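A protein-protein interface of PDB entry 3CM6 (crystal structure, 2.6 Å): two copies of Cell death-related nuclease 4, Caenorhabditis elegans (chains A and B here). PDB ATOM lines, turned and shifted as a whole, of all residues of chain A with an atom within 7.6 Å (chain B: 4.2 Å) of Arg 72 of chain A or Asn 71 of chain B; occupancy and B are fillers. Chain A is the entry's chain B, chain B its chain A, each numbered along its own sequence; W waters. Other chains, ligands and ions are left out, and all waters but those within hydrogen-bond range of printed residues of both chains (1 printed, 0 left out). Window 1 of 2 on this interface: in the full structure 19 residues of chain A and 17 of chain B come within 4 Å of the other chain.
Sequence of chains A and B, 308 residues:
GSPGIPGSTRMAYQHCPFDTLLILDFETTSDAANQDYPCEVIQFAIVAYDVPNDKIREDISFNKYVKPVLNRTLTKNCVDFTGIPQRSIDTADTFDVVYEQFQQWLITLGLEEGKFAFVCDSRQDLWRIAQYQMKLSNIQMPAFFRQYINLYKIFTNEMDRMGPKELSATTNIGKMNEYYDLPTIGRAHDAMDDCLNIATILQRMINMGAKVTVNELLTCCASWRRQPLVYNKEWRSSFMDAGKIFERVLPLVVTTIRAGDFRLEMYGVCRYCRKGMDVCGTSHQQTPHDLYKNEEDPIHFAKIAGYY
Tyr 37 of chain A touches Thr 73 of chain B, and with the chains exchanged Thr 73 of chain A touches Tyr 37 of chain B.
Leu 70 of chain A touches Arg 72 of chain B, and with the chains exchanged Arg 72 of chain A touches Leu 70 of chain B.
Asn 71 of chain A touches Arg 72 of chain B, and with the chains exchanged Arg 72 of chain A touches Asn 71 of chain B.
Arg 72 of chain A touches Val 69 of chain B, but with the chains exchanged Val 69 of chain A does not touch Arg 72 of chain B (5.3 Å).
Positions printed for both chains: 29, 37, 40, 68, 69, 70, 71, 72 and 73.
Of the 16 pairs that touch across the chains among the printed residues, 13 have their exchanged pair printed and touching as well.
Hydrophobic or aromatic side chains of chain B that line the printed part of chain A: Tyr 37 and Pro 38.
Along chain B the printed residues that touch a printed residue of chain A span positions 37 to 73.
Of the 18 printed residues of chain A, 7 touch a printed residue of chain B.
Printed residues of chain A that touch a printed residue of chain B: Tyr 37, Val 69, Leu 70, Asn 71, Arg 72, Thr 73 and Ile 304.
Hydrophobic or aromatic side chains of chain A within 4 Å of the printed part of chain B: Tyr 37 and Ile 304.
Among the printed residues, no Asp or Glu carboxylate lies within 4 Å of a Lys or Arg side-chain nitrogen of the other chain.
N of Asn 71 of chain B lies within hydrogen-bond range of OE1 of Glu 40 of chain B (3.2 Å).
N of Leu 70 of chain B lies within hydrogen-bond range of OE1 of Glu 40 of chain B.
The side-chain carboxylate of Glu 40 of chain A sits at hydrogen-bond distance from the backbone NH of Asn 71 of chain A (3.1 Å).
The backbone carbonyl oxygen (O) of Arg 72 of chain A sits at hydrogen-bond distance from the side-chain amide nitrogen (NE2) of Gln 86 of chain A (3.0 Å).
The guanidinium group (NH2) of Arg 72 of chain A is in hydrogen-bond range of the backbone carbonyl oxygen (O) of Val 69 of chain A (3.0 Å).
The side-chain carboxylate of Glu 40 of chain B sits at hydrogen-bond distance from the backbone NH of Val 69 of chain B, at 2.7 Å.
Of chain B, only Val 69 (3.3 Å), Leu 70 (3.0 Å) and Asn 71 (3.6 Å) come within 4 Å of Arg 72 of chain A.
Asn 71 of chain B touches four residues of chain A.
Of the printed residues of chain A, Tyr 37 of chain B touches Thr 73 (3.8 Å).
Of the printed residues of chain B, Ile 304 of chain A touches Arg 72.
Of the printed residues of chain A, Thr 73 of chain B touches Tyr 37 (3.7 Å) and Asn 71 (3.0 Å).
Of the printed residues of chain A, Arg 72 of chain B touches Leu 70 (2.9 Å), Asn 71 (3.1 Å) and Ile 304 (3.8 Å).
The nearest printed residue of chain B that does not touch Arg 72 of chain A is Arg 72 of chain B (6.0 Å).
The nearest printed residue of chain A that does not touch Thr 73 of chain B is Ile 304 of chain A (4.7 Å).
O of Leu 70 of chain A sits at hydrogen-bond distance from N of Arg 72 of chain B (2.9 Å).
The side-chain amide oxygen of Asn 71 of chain B is in hydrogen-bond range of the side-chain hydroxyl of Thr 73 of chain A (3.1 Å).
OD1 of Asn 71 of chain A lies within hydrogen-bond range of OG1 of Thr 73 of chain B, at 3.0 Å.
The backbone carbonyl oxygen of Leu 70 of chain B sits at hydrogen-bond distance from the backbone NH of Arg 72 of chain A (3.0 Å).
The backbone carbonyl oxygen (O) of Leu 70 of chain B sits close to the backbone carbonyl oxygen (O) of Leu 70 of chain A, at 2.9 Å.
The guanidinium group (NH2) of Arg 72 of chain A is in hydrogen-bond range of the backbone carbonyl oxygen (O) of Val 69 of chain B (3.3 Å).
N of Arg 72 of chain B sits close to ND2 of Asn 71 of chain A (3.1 Å).
Water W1 lies within hydrogen-bond range of ND2 of Asn 71 of chain B (2.4 Å) and ND2 of Asn 71 of chain A (2.5 Å).
CG2 of Thr 73 of chain B touches CD1 of Tyr 37 of chain A, 3.7 Å away.
Val 69 of chain A touches Val 69 of chain B.
Leu 70 of chain A touches Asn 71 of chain B.
CA of Asn 71 of chain A touches O of Leu 70 of chain B (3.5 Å).
Asn 71 of chain A touches Asn 71 of chain B.
Asn 71 of chain B touches Arg 72 of chain A.
CD1 of Tyr 37 of chain B touches CG2 of Thr 73 of chain A, at 3.8 Å.
Thr 73 of chain A touches Pro 38 of chain B (OG1 to CG, 3.1 Å).
CB of Arg 72 of chain B touches CD1 of Ile 304 of chain A (3.8 Å).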
ATOM      1  N   THR A  29       9.984  -1.959  13.633  1.00  0.00           N
ATOM      2  CA  THR A  29       9.222  -0.786  14.018  1.00  0.00           C
ATOM      3  C   THR A  29       8.964   0.016  12.750  1.00  0.00           C
ATOM      4  O   THR A  29       9.793   0.012  11.829  1.00  0.00           O
ATOM      5  CB  THR A  29      10.008   0.107  14.971  1.00  0.00           C
ATOM      6  OG1 THR A  29      11.218   0.537  14.329  1.00  0.00           O
ATOM      7  CG2 THR A  29      10.353  -0.622  16.232  1.00  0.00           C
ATOM      8  N   TYR A  37      12.184   7.159   9.168  1.00  0.00           N
ATOM      9  CA  TYR A  37      11.970   6.421  10.380  1.00  0.00           C
ATOM     10  C   TYR A  37      13.152   5.483  10.624  1.00  0.00           C
ATOM     11  O   TYR A  37      13.582   4.821   9.712  1.00  0.00           O
ATOM     12  CB  TYR A  37      10.657   5.645  10.245  1.00  0.00           C
ATOM     13  CG  TYR A  37      10.181   5.104  11.553  1.00  0.00           C
ATOM     14  CD1 TYR A  37       9.385   5.873  12.394  1.00  0.00           C
ATOM     15  CD2 TYR A  37      10.539   3.829  11.966  1.00  0.00           C
ATOM     16  CE1 TYR A  37       8.957   5.386  13.599  1.00  0.00           C
ATOM     17  CE2 TYR A  37      10.108   3.330  13.187  1.00  0.00           C
ATOM     18  CZ  TYR A  37       9.321   4.118  13.993  1.00  0.00           C
ATOM     19  OH  TYR A  37       8.904   3.634  15.200  1.00  0.00           O
ATOM     20  N   GLU A  40      13.849  -0.469  13.571  1.00  0.00           N
ATOM     21  CA  GLU A  40      14.535  -1.393  14.434  1.00  0.00           C
ATOM     22  C   GLU A  40      13.842  -2.730  14.307  1.00  0.00           C
ATOM     23  O   GLU A  40      12.607  -2.795  14.220  1.00  0.00           O
ATOM     24  CB  GLU A  40      14.493  -0.905  15.881  1.00  0.00           C
ATOM     25  CG  GLU A  40      15.403   0.289  16.148  1.00  0.00           C
ATOM     26  CD  GLU A  40      15.219   0.821  17.539  1.00  0.00           C
ATOM     27  OE1 GLU A  40      14.131   1.381  17.809  1.00  0.00           O
ATOM     28  OE2 GLU A  40      16.144   0.668  18.375  1.00  0.00           O
ATOM     29  N   ILE A  42      12.081  -5.958  15.199  1.00  0.00           N
ATOM     30  CA  ILE A  42      11.263  -6.432  16.305  1.00  0.00           C
ATOM     31  C   ILE A  42      10.920  -7.929  16.217  1.00  0.00           C
ATOM     32  O   ILE A  42      10.352  -8.502  17.158  1.00  0.00           O
ATOM     33  CB  ILE A  42       9.994  -5.590  16.506  1.00  0.00           C
ATOM     34  CG1 ILE A  42       9.136  -5.532  15.242  1.00  0.00           C
ATOM     35  CG2 ILE A  42      10.359  -4.201  17.016  1.00  0.00           C
ATOM     36  CD1 ILE A  42       7.846  -4.737  15.439  1.00  0.00           C
ATOM     37  N   LYS A  67      13.453  -6.421  21.317  1.00  0.00           N
ATOM     38  CA  LYS A  67      13.077  -5.155  21.945  1.00  0.00           C
ATOM     39  C   LYS A  67      13.878  -3.967  21.373  1.00  0.00           C
ATOM     40  O   LYS A  67      15.104  -3.932  21.500  1.00  0.00           O
ATOM     41  CB  LYS A  67      13.291  -5.251  23.464  1.00  0.00           C
ATOM     42  CG  LYS A  67      12.767  -4.047  24.279  1.00  0.00           C
ATOM     43  CD  LYS A  67      12.792  -4.341  25.802  1.00  0.00           C
ATOM     44  CE  LYS A  67      14.156  -3.998  26.401  1.00  0.00           C
ATOM     45  NZ  LYS A  67      14.577  -4.901  27.515  1.00  0.00           N
ATOM     46  N   PRO A  68      13.196  -2.984  20.757  1.00  0.00           N
ATOM     47  CA  PRO A  68      13.881  -1.794  20.227  1.00  0.00           C
ATOM     48  C   PRO A  68      14.458  -0.931  21.336  1.00  0.00           C
ATOM     49  O   PRO A  68      14.056  -1.073  22.500  1.00  0.00           O
ATOM     50  CB  PRO A  68      12.766  -1.014  19.535  1.00  0.00           C
ATOM     51  CG  PRO A  68      11.636  -1.959  19.396  1.00  0.00           C
ATOM     52  CD  PRO A  68      11.745  -2.917  20.524  1.00  0.00           C
ATOM     53  N   VAL A  69      15.398  -0.051  20.992  1.00  0.00           N
ATOM     54  CA  VAL A  69      15.921   0.884  21.984  1.00  0.00           C
ATOM     55  C   VAL A  69      15.556   2.339  21.652  1.00  0.00           C
ATOM     56  O   VAL A  69      15.555   3.195  22.548  1.00  0.00           O
ATOM     57  CB  VAL A  69      17.455   0.707  22.249  1.00  0.00           C
ATOM     58  CG1 VAL A  69      17.811  -0.787  22.439  1.00  0.00           C
ATOM     59  CG2 VAL A  69      18.295   1.305  21.134  1.00  0.00           C
ATOM     60  N   LEU A  70      15.235   2.613  20.388  1.00  0.00           N
ATOM     61  CA  LEU A  70      14.938   3.980  19.953  1.00  0.00           C
ATOM     62  C   LEU A  70      13.447   4.307  20.038  1.00  0.00           C
ATOM     63  O   LEU A  70      13.060   5.386  20.480  1.00  0.00           O
ATOM     64  CB  LEU A  70      15.441   4.209  18.517  1.00  0.00           C
ATOM     65  CG  LEU A  70      16.857   4.764  18.259  1.00  0.00           C
ATOM     66  CD1 LEU A  70      17.858   4.458  19.368  1.00  0.00           C
ATOM     67  CD2 LEU A  70      17.384   4.300  16.910  1.00  0.00           C
ATOM     68  N   ASN A  71      12.625   3.376  19.567  1.00  0.00           N
ATOM     69  CA  ASN A  71      11.190   3.492  19.632  1.00  0.00           C
ATOM     70  C   ASN A  71      10.603   2.244  20.235  1.00  0.00           C
ATOM     71  O   ASN A  71      10.191   1.307  19.542  1.00  0.00           O
ATOM     72  CB  ASN A  71      10.604   3.805  18.272  1.00  0.00           C
ATOM     73  CG  ASN A  71      10.922   5.205  17.844  1.00  0.00           C
ATOM     74  OD1 ASN A  71      11.710   5.419  16.911  1.00  0.00           O
ATOM     75  ND2 ASN A  71      10.334   6.191  18.547  1.00  0.00           N
ATOM     76  N   ARG A  72      10.569   2.282  21.560  1.00  0.00           N
ATOM     77  CA  ARG A  72      10.168   1.172  22.388  1.00  0.00           C
ATOM     78  C   ARG A  72       8.695   0.869  22.365  1.00  0.00           C
ATOM     79  O   ARG A  72       8.307  -0.248  22.666  1.00  0.00           O
ATOM     80  CB  ARG A  72      10.611   1.451  23.802  1.00  0.00           C
ATOM     81  CG  ARG A  72      11.952   0.868  24.060  1.00  0.00           C
ATOM     82  CD  ARG A  72      12.532   1.416  25.277  1.00  0.00           C
ATOM     83  NE  ARG A  72      13.641   2.302  24.980  1.00  0.00           N
ATOM     84  CZ  ARG A  72      14.620   2.551  25.843  1.00  0.00           C
ATOM     85  NH1 ARG A  72      14.606   1.975  27.043  1.00  0.00           N
ATOM     86  NH2 ARG A  72      15.601   3.378  25.512  1.00  0.00           N
ATOM     87  N   THR A  73       7.880   1.844  21.985  1.00  0.00           N
ATOM     88  CA  THR A  73       6.444   1.653  21.921  1.00  0.00           C
ATOM     89  C   THR A  73       6.002   1.507  20.479  1.00  0.00           C
ATOM     90  O   THR A  73       6.174   2.418  19.665  1.00  0.00           O
ATOM     91  CB  THR A  73       5.684   2.827  22.603  1.00  0.00           C
ATOM     92  OG1 THR A  73       6.111   2.944  23.967  1.00  0.00           O
ATOM     93  CG2 THR A  73       4.182   2.609  22.566  1.00  0.00           C
ATOM     94  N   LEU A  74       5.420   0.364  20.162  1.00  0.00           N
ATOM     95  CA  LEU A  74       4.987   0.094  18.805  1.00  0.00           C
ATOM     96  C   LEU A  74       3.840   1.005  18.431  1.00  0.00           C
ATOM     97  O   LEU A  74       2.832   1.105  19.119  1.00  0.00           O
ATOM     98  CB  LEU A  74       4.587  -1.374  18.630  1.00  0.00           C
ATOM     99  CG  LEU A  74       5.605  -2.398  18.129  1.00  0.00           C
ATOM    100  CD1 LEU A  74       7.020  -2.182  18.649  1.00  0.00           C
ATOM    101  CD2 LEU A  74       5.141  -3.816  18.449  1.00  0.00           C
ATOM    102  N   THR A  75       4.044   1.709  17.342  1.00  0.00           N
ATOM    103  CA  THR A  75       2.997   2.426  16.650  1.00  0.00           C
ATOM    104  C   THR A  75       1.784   1.508  16.472  1.00  0.00           C
ATOM    105  O   THR A  75       1.925   0.316  16.201  1.00  0.00           O
ATOM    106  CB  THR A  75       3.573   2.886  15.307  1.00  0.00           C
ATOM    107  OG1 THR A  75       4.043   4.233  15.447  1.00  0.00           O
ATOM    108  CG2 THR A  75       2.581   2.822  14.211  1.00  0.00           C
ATOM    109  N   GLN A  86       2.372  -5.320  21.733  1.00  0.00           N
ATOM    110  CA  GLN A  86       3.342  -4.689  22.626  1.00  0.00           C
ATOM    111  C   GLN A  86       3.919  -5.618  23.714  1.00  0.00           C
ATOM    112  O   GLN A  86       5.106  -5.529  24.031  1.00  0.00           O
ATOM    113  CB  GLN A  86       2.761  -3.399  23.230  1.00  0.00           C
ATOM    114  CG  GLN A  86       3.770  -2.553  23.981  1.00  0.00           C
ATOM    115  CD  GLN A  86       4.888  -2.004  23.072  1.00  0.00           C
ATOM    116  OE1 GLN A  86       4.617  -1.481  21.988  1.00  0.00           O
ATOM    117  NE2 GLN A  86       6.135  -2.119  23.521  1.00  0.00           N
ATOM    118  N   ILE A  89       7.146  -7.582  22.654  1.00  0.00           N
ATOM    119  CA  ILE A  89       8.389  -6.829  22.577  1.00  0.00           C
ATOM    120  C   ILE A  89       8.917  -6.350  23.956  1.00  0.00           C
ATOM    121  O   ILE A  89      10.129  -6.214  24.137  1.00  0.00           O
ATOM    122  CB  ILE A  89       8.368  -5.719  21.471  1.00  0.00           C
ATOM    123  CG1 ILE A  89       7.986  -4.375  22.037  1.00  0.00           C
ATOM    124  CG2 ILE A  89       7.491  -6.105  20.279  1.00  0.00           C
ATOM    125  CD1 ILE A  89       9.178  -3.573  22.475  1.00  0.00           C
ATOM    126  N   ASP A  90       8.023  -6.134  24.925  1.00  0.00           N
ATOM    127  CA  ASP A  90       8.439  -5.708  26.279  1.00  0.00           C
ATOM    128  C   ASP A  90       9.138  -6.842  27.055  1.00  0.00           C
ATOM    129  O   ASP A  90       9.932  -6.589  27.971  1.00  0.00           O
ATOM    130  CB  ASP A  90       7.266  -5.151  27.103  1.00  0.00           C
ATOM    131  CG  ASP A  90       6.797  -3.753  26.643  1.00  0.00           C
ATOM    132  OD1 ASP A  90       5.942  -3.178  27.341  1.00  0.00           O
ATOM    133  OD2 ASP A  90       7.256  -3.214  25.609  1.00  0.00           O
ATOM    134  N   THR A  94      17.128  -7.184  23.657  1.00  0.00           N
ATOM    135  CA  THR A  94      17.524  -6.209  22.646  1.00  0.00           C
ATOM    136  C   THR A  94      18.228  -6.927  21.486  1.00  0.00           C
ATOM    137  O   THR A  94      18.526  -8.130  21.576  1.00  0.00           O
ATOM    138  CB  THR A  94      18.425  -5.088  23.233  1.00  0.00           C
ATOM    139  OG1 THR A  94      19.375  -5.666  24.128  1.00  0.00           O
ATOM    140  CG2 THR A  94      17.599  -4.080  23.991  1.00  0.00           C
ATOM    141  N   ILE A 304      20.082  10.001  13.687  1.00  0.00           N
ATOM    142  CA  ILE A 304      19.954   9.169  14.882  1.00  0.00           C
ATOM    143  C   ILE A 304      20.898   7.955  14.864  1.00  0.00           C
ATOM    144  O   ILE A 304      21.263   7.456  15.916  1.00  0.00           O
ATOM    145  CB  ILE A 304      18.474   8.753  15.131  1.00  0.00           C
ATOM    146  CG1 ILE A 304      18.243   8.491  16.613  1.00  0.00           C
ATOM    147  CG2 ILE A 304      18.063   7.560  14.225  1.00  0.00           C
ATOM    148  CD1 ILE A 304      16.774   8.378  16.983  1.00  0.00           C
ATOM    149  N   THR B  29       5.082  13.463  23.435  1.00  0.00           N
ATOM    150  CA  THR B  29       4.982  12.389  22.456  1.00  0.00           C
ATOM    151  C   THR B  29       3.619  11.741  22.642  1.00  0.00           C
ATOM    152  O   THR B  29       3.097  11.683  23.752  1.00  0.00           O
ATOM    153  CB  THR B  29       6.034  11.293  22.698  1.00  0.00           C
ATOM    154  OG1 THR B  29       5.880  10.764  24.024  1.00  0.00           O
ATOM    155  CG2 THR B  29       7.453  11.808  22.521  1.00  0.00           C
ATOM    156  N   TYR B  37       0.223   4.435  26.199  1.00  0.00           N
ATOM    157  CA  TYR B  37       1.372   5.120  25.642  1.00  0.00           C
ATOM    158  C   TYR B  37       2.149   5.814  26.755  1.00  0.00           C
ATOM    159  O   TYR B  37       1.543   6.485  27.600  1.00  0.00           O
ATOM    160  CB  TYR B  37       0.889   6.147  24.615  1.00  0.00           C
ATOM    161  CG  TYR B  37       2.000   6.628  23.752  1.00  0.00           C
ATOM    162  CD1 TYR B  37       2.313   5.968  22.561  1.00  0.00           C
ATOM    163  CD2 TYR B  37       2.778   7.721  24.133  1.00  0.00           C
ATOM    164  CE1 TYR B  37       3.357   6.399  21.761  1.00  0.00           C
ATOM    165  CE2 TYR B  37       3.831   8.154  23.336  1.00  0.00           C
ATOM    166  CZ  TYR B  37       4.107   7.486  22.161  1.00  0.00           C
ATOM    167  OH  TYR B  37       5.134   7.906  21.392  1.00  0.00           O
ATOM    168  N   PRO B  38       3.488   5.659  26.763  1.00  0.00           N
ATOM    169  CA  PRO B  38       4.371   6.298  27.743  1.00  0.00           C
ATOM    170  C   PRO B  38       4.716   7.757  27.392  1.00  0.00           C
ATOM    171  O   PRO B  38       5.868   8.074  27.091  1.00  0.00           O
ATOM    172  CB  PRO B  38       5.624   5.442  27.669  1.00  0.00           C
ATOM    173  CG  PRO B  38       5.650   4.937  26.265  1.00  0.00           C
ATOM    174  CD  PRO B  38       4.237   4.830  25.804  1.00  0.00           C
ATOM    175  N   GLU B  40       5.960  11.284  26.857  1.00  0.00           N
ATOM    176  CA  GLU B  40       7.182  11.955  27.260  1.00  0.00           C
ATOM    177  C   GLU B  40       7.096  13.411  26.861  1.00  0.00           C
ATOM    178  O   GLU B  40       6.564  13.726  25.798  1.00  0.00           O
ATOM    179  CB  GLU B  40       8.390  11.288  26.604  1.00  0.00           C
ATOM    180  CG  GLU B  40       8.932  10.090  27.382  1.00  0.00           C
ATOM    181  CD  GLU B  40      10.151   9.469  26.703  1.00  0.00           C
ATOM    182  OE1 GLU B  40       9.974   8.823  25.645  1.00  0.00           O
ATOM    183  OE2 GLU B  40      11.283   9.635  27.220  1.00  0.00           O
ATOM    184  N   PRO B  68      12.952  12.931  23.950  1.00  0.00           N
ATOM    185  CA  PRO B  68      12.489  11.692  24.625  1.00  0.00           C
ATOM    186  C   PRO B  68      13.591  10.621  24.706  1.00  0.00           C
ATOM    187  O   PRO B  68      14.626  10.753  24.060  1.00  0.00           O
ATOM    188  CB  PRO B  68      11.367  11.197  23.720  1.00  0.00           C
ATOM    189  CG  PRO B  68      11.131  12.315  22.705  1.00  0.00           C
ATOM    190  CD  PRO B  68      12.372  13.093  22.612  1.00  0.00           C
ATOM    191  N   VAL B  69      13.403   9.591  25.522  1.00  0.00           N
ATOM    192  CA  VAL B  69      14.332   8.463  25.497  1.00  0.00           C
ATOM    193  C   VAL B  69      13.634   7.163  25.144  1.00  0.00           C
ATOM    194  O   VAL B  69      14.258   6.282  24.570  1.00  0.00           O
ATOM    195  CB  VAL B  69      15.241   8.322  26.789  1.00  0.00           C
ATOM    196  CG1 VAL B  69      15.446   9.652  27.487  1.00  0.00           C
ATOM    197  CG2 VAL B  69      14.714   7.277  27.758  1.00  0.00           C
ATOM    198  N   LEU B  70      12.342   7.053  25.442  1.00  0.00           N
ATOM    199  CA  LEU B  70      11.576   5.858  25.057  1.00  0.00           C
ATOM    200  C   LEU B  70      11.193   5.866  23.591  1.00  0.00           C
ATOM    201  O   LEU B  70      11.430   4.885  22.875  1.00  0.00           O
ATOM    202  CB  LEU B  70      10.320   5.682  25.925  1.00  0.00           C
ATOM    203  CG  LEU B  70      10.466   5.736  27.455  1.00  0.00           C
ATOM    204  CD1 LEU B  70       9.166   5.255  28.072  1.00  0.00           C
ATOM    205  CD2 LEU B  70      11.642   4.922  28.007  1.00  0.00           C
ATOM    206  N   ASN B  71      10.588   6.968  23.152  1.00  0.00           N
ATOM    207  CA  ASN B  71      10.147   7.115  21.778  1.00  0.00           C
ATOM    208  C   ASN B  71      10.801   8.319  21.087  1.00  0.00           C
ATOM    209  O   ASN B  71      10.272   9.444  21.099  1.00  0.00           O
ATOM    210  CB  ASN B  71       8.623   7.143  21.695  1.00  0.00           C
ATOM    211  CG  ASN B  71       7.996   5.782  22.009  1.00  0.00           C
ATOM    212  OD1 ASN B  71       7.418   5.599  23.076  1.00  0.00           O
ATOM    213  ND2 ASN B  71       8.117   4.818  21.083  1.00  0.00           N
ATOM    214  N   ARG B  72      11.951   8.057  20.467  1.00  0.00           N
ATOM    215  CA  ARG B  72      12.797   9.116  19.932  1.00  0.00           C
ATOM    216  C   ARG B  72      12.301   9.747  18.638  1.00  0.00           C
ATOM    217  O   ARG B  72      12.637  10.893  18.335  1.00  0.00           O
ATOM    218  CB  ARG B  72      14.253   8.654  19.836  1.00  0.00           C
ATOM    219  CG  ARG B  72      14.854   8.453  21.221  1.00  0.00           C
ATOM    220  CD  ARG B  72      16.352   8.215  21.226  1.00  0.00           C
ATOM    221  NE  ARG B  72      17.094   9.366  20.697  1.00  0.00           N
ATOM    222  CZ  ARG B  72      18.422   9.410  20.551  1.00  0.00           C
ATOM    223  NH1 ARG B  72      19.168   8.368  20.909  1.00  0.00           N
ATOM    224  NH2 ARG B  72      19.004  10.504  20.059  1.00  0.00           N
ATOM    225  N   THR B  73      11.483   9.014  17.900  1.00  0.00           N
ATOM    226  CA  THR B  73      10.908   9.495  16.653  1.00  0.00           C
ATOM    227  C   THR B  73       9.437   9.847  16.849  1.00  0.00           C
ATOM    228  O   THR B  73       8.625   8.961  17.118  1.00  0.00           O
ATOM    229  CB  THR B  73      10.997   8.402  15.566  1.00  0.00           C
ATOM    230  OG1 THR B  73      12.352   7.989  15.446  1.00  0.00           O
ATOM    231  CG2 THR B  73      10.517   8.902  14.228  1.00  0.00           C
HETATM  232  O   HOH W   1       7.941   5.747  18.859  1.00  0.00           O
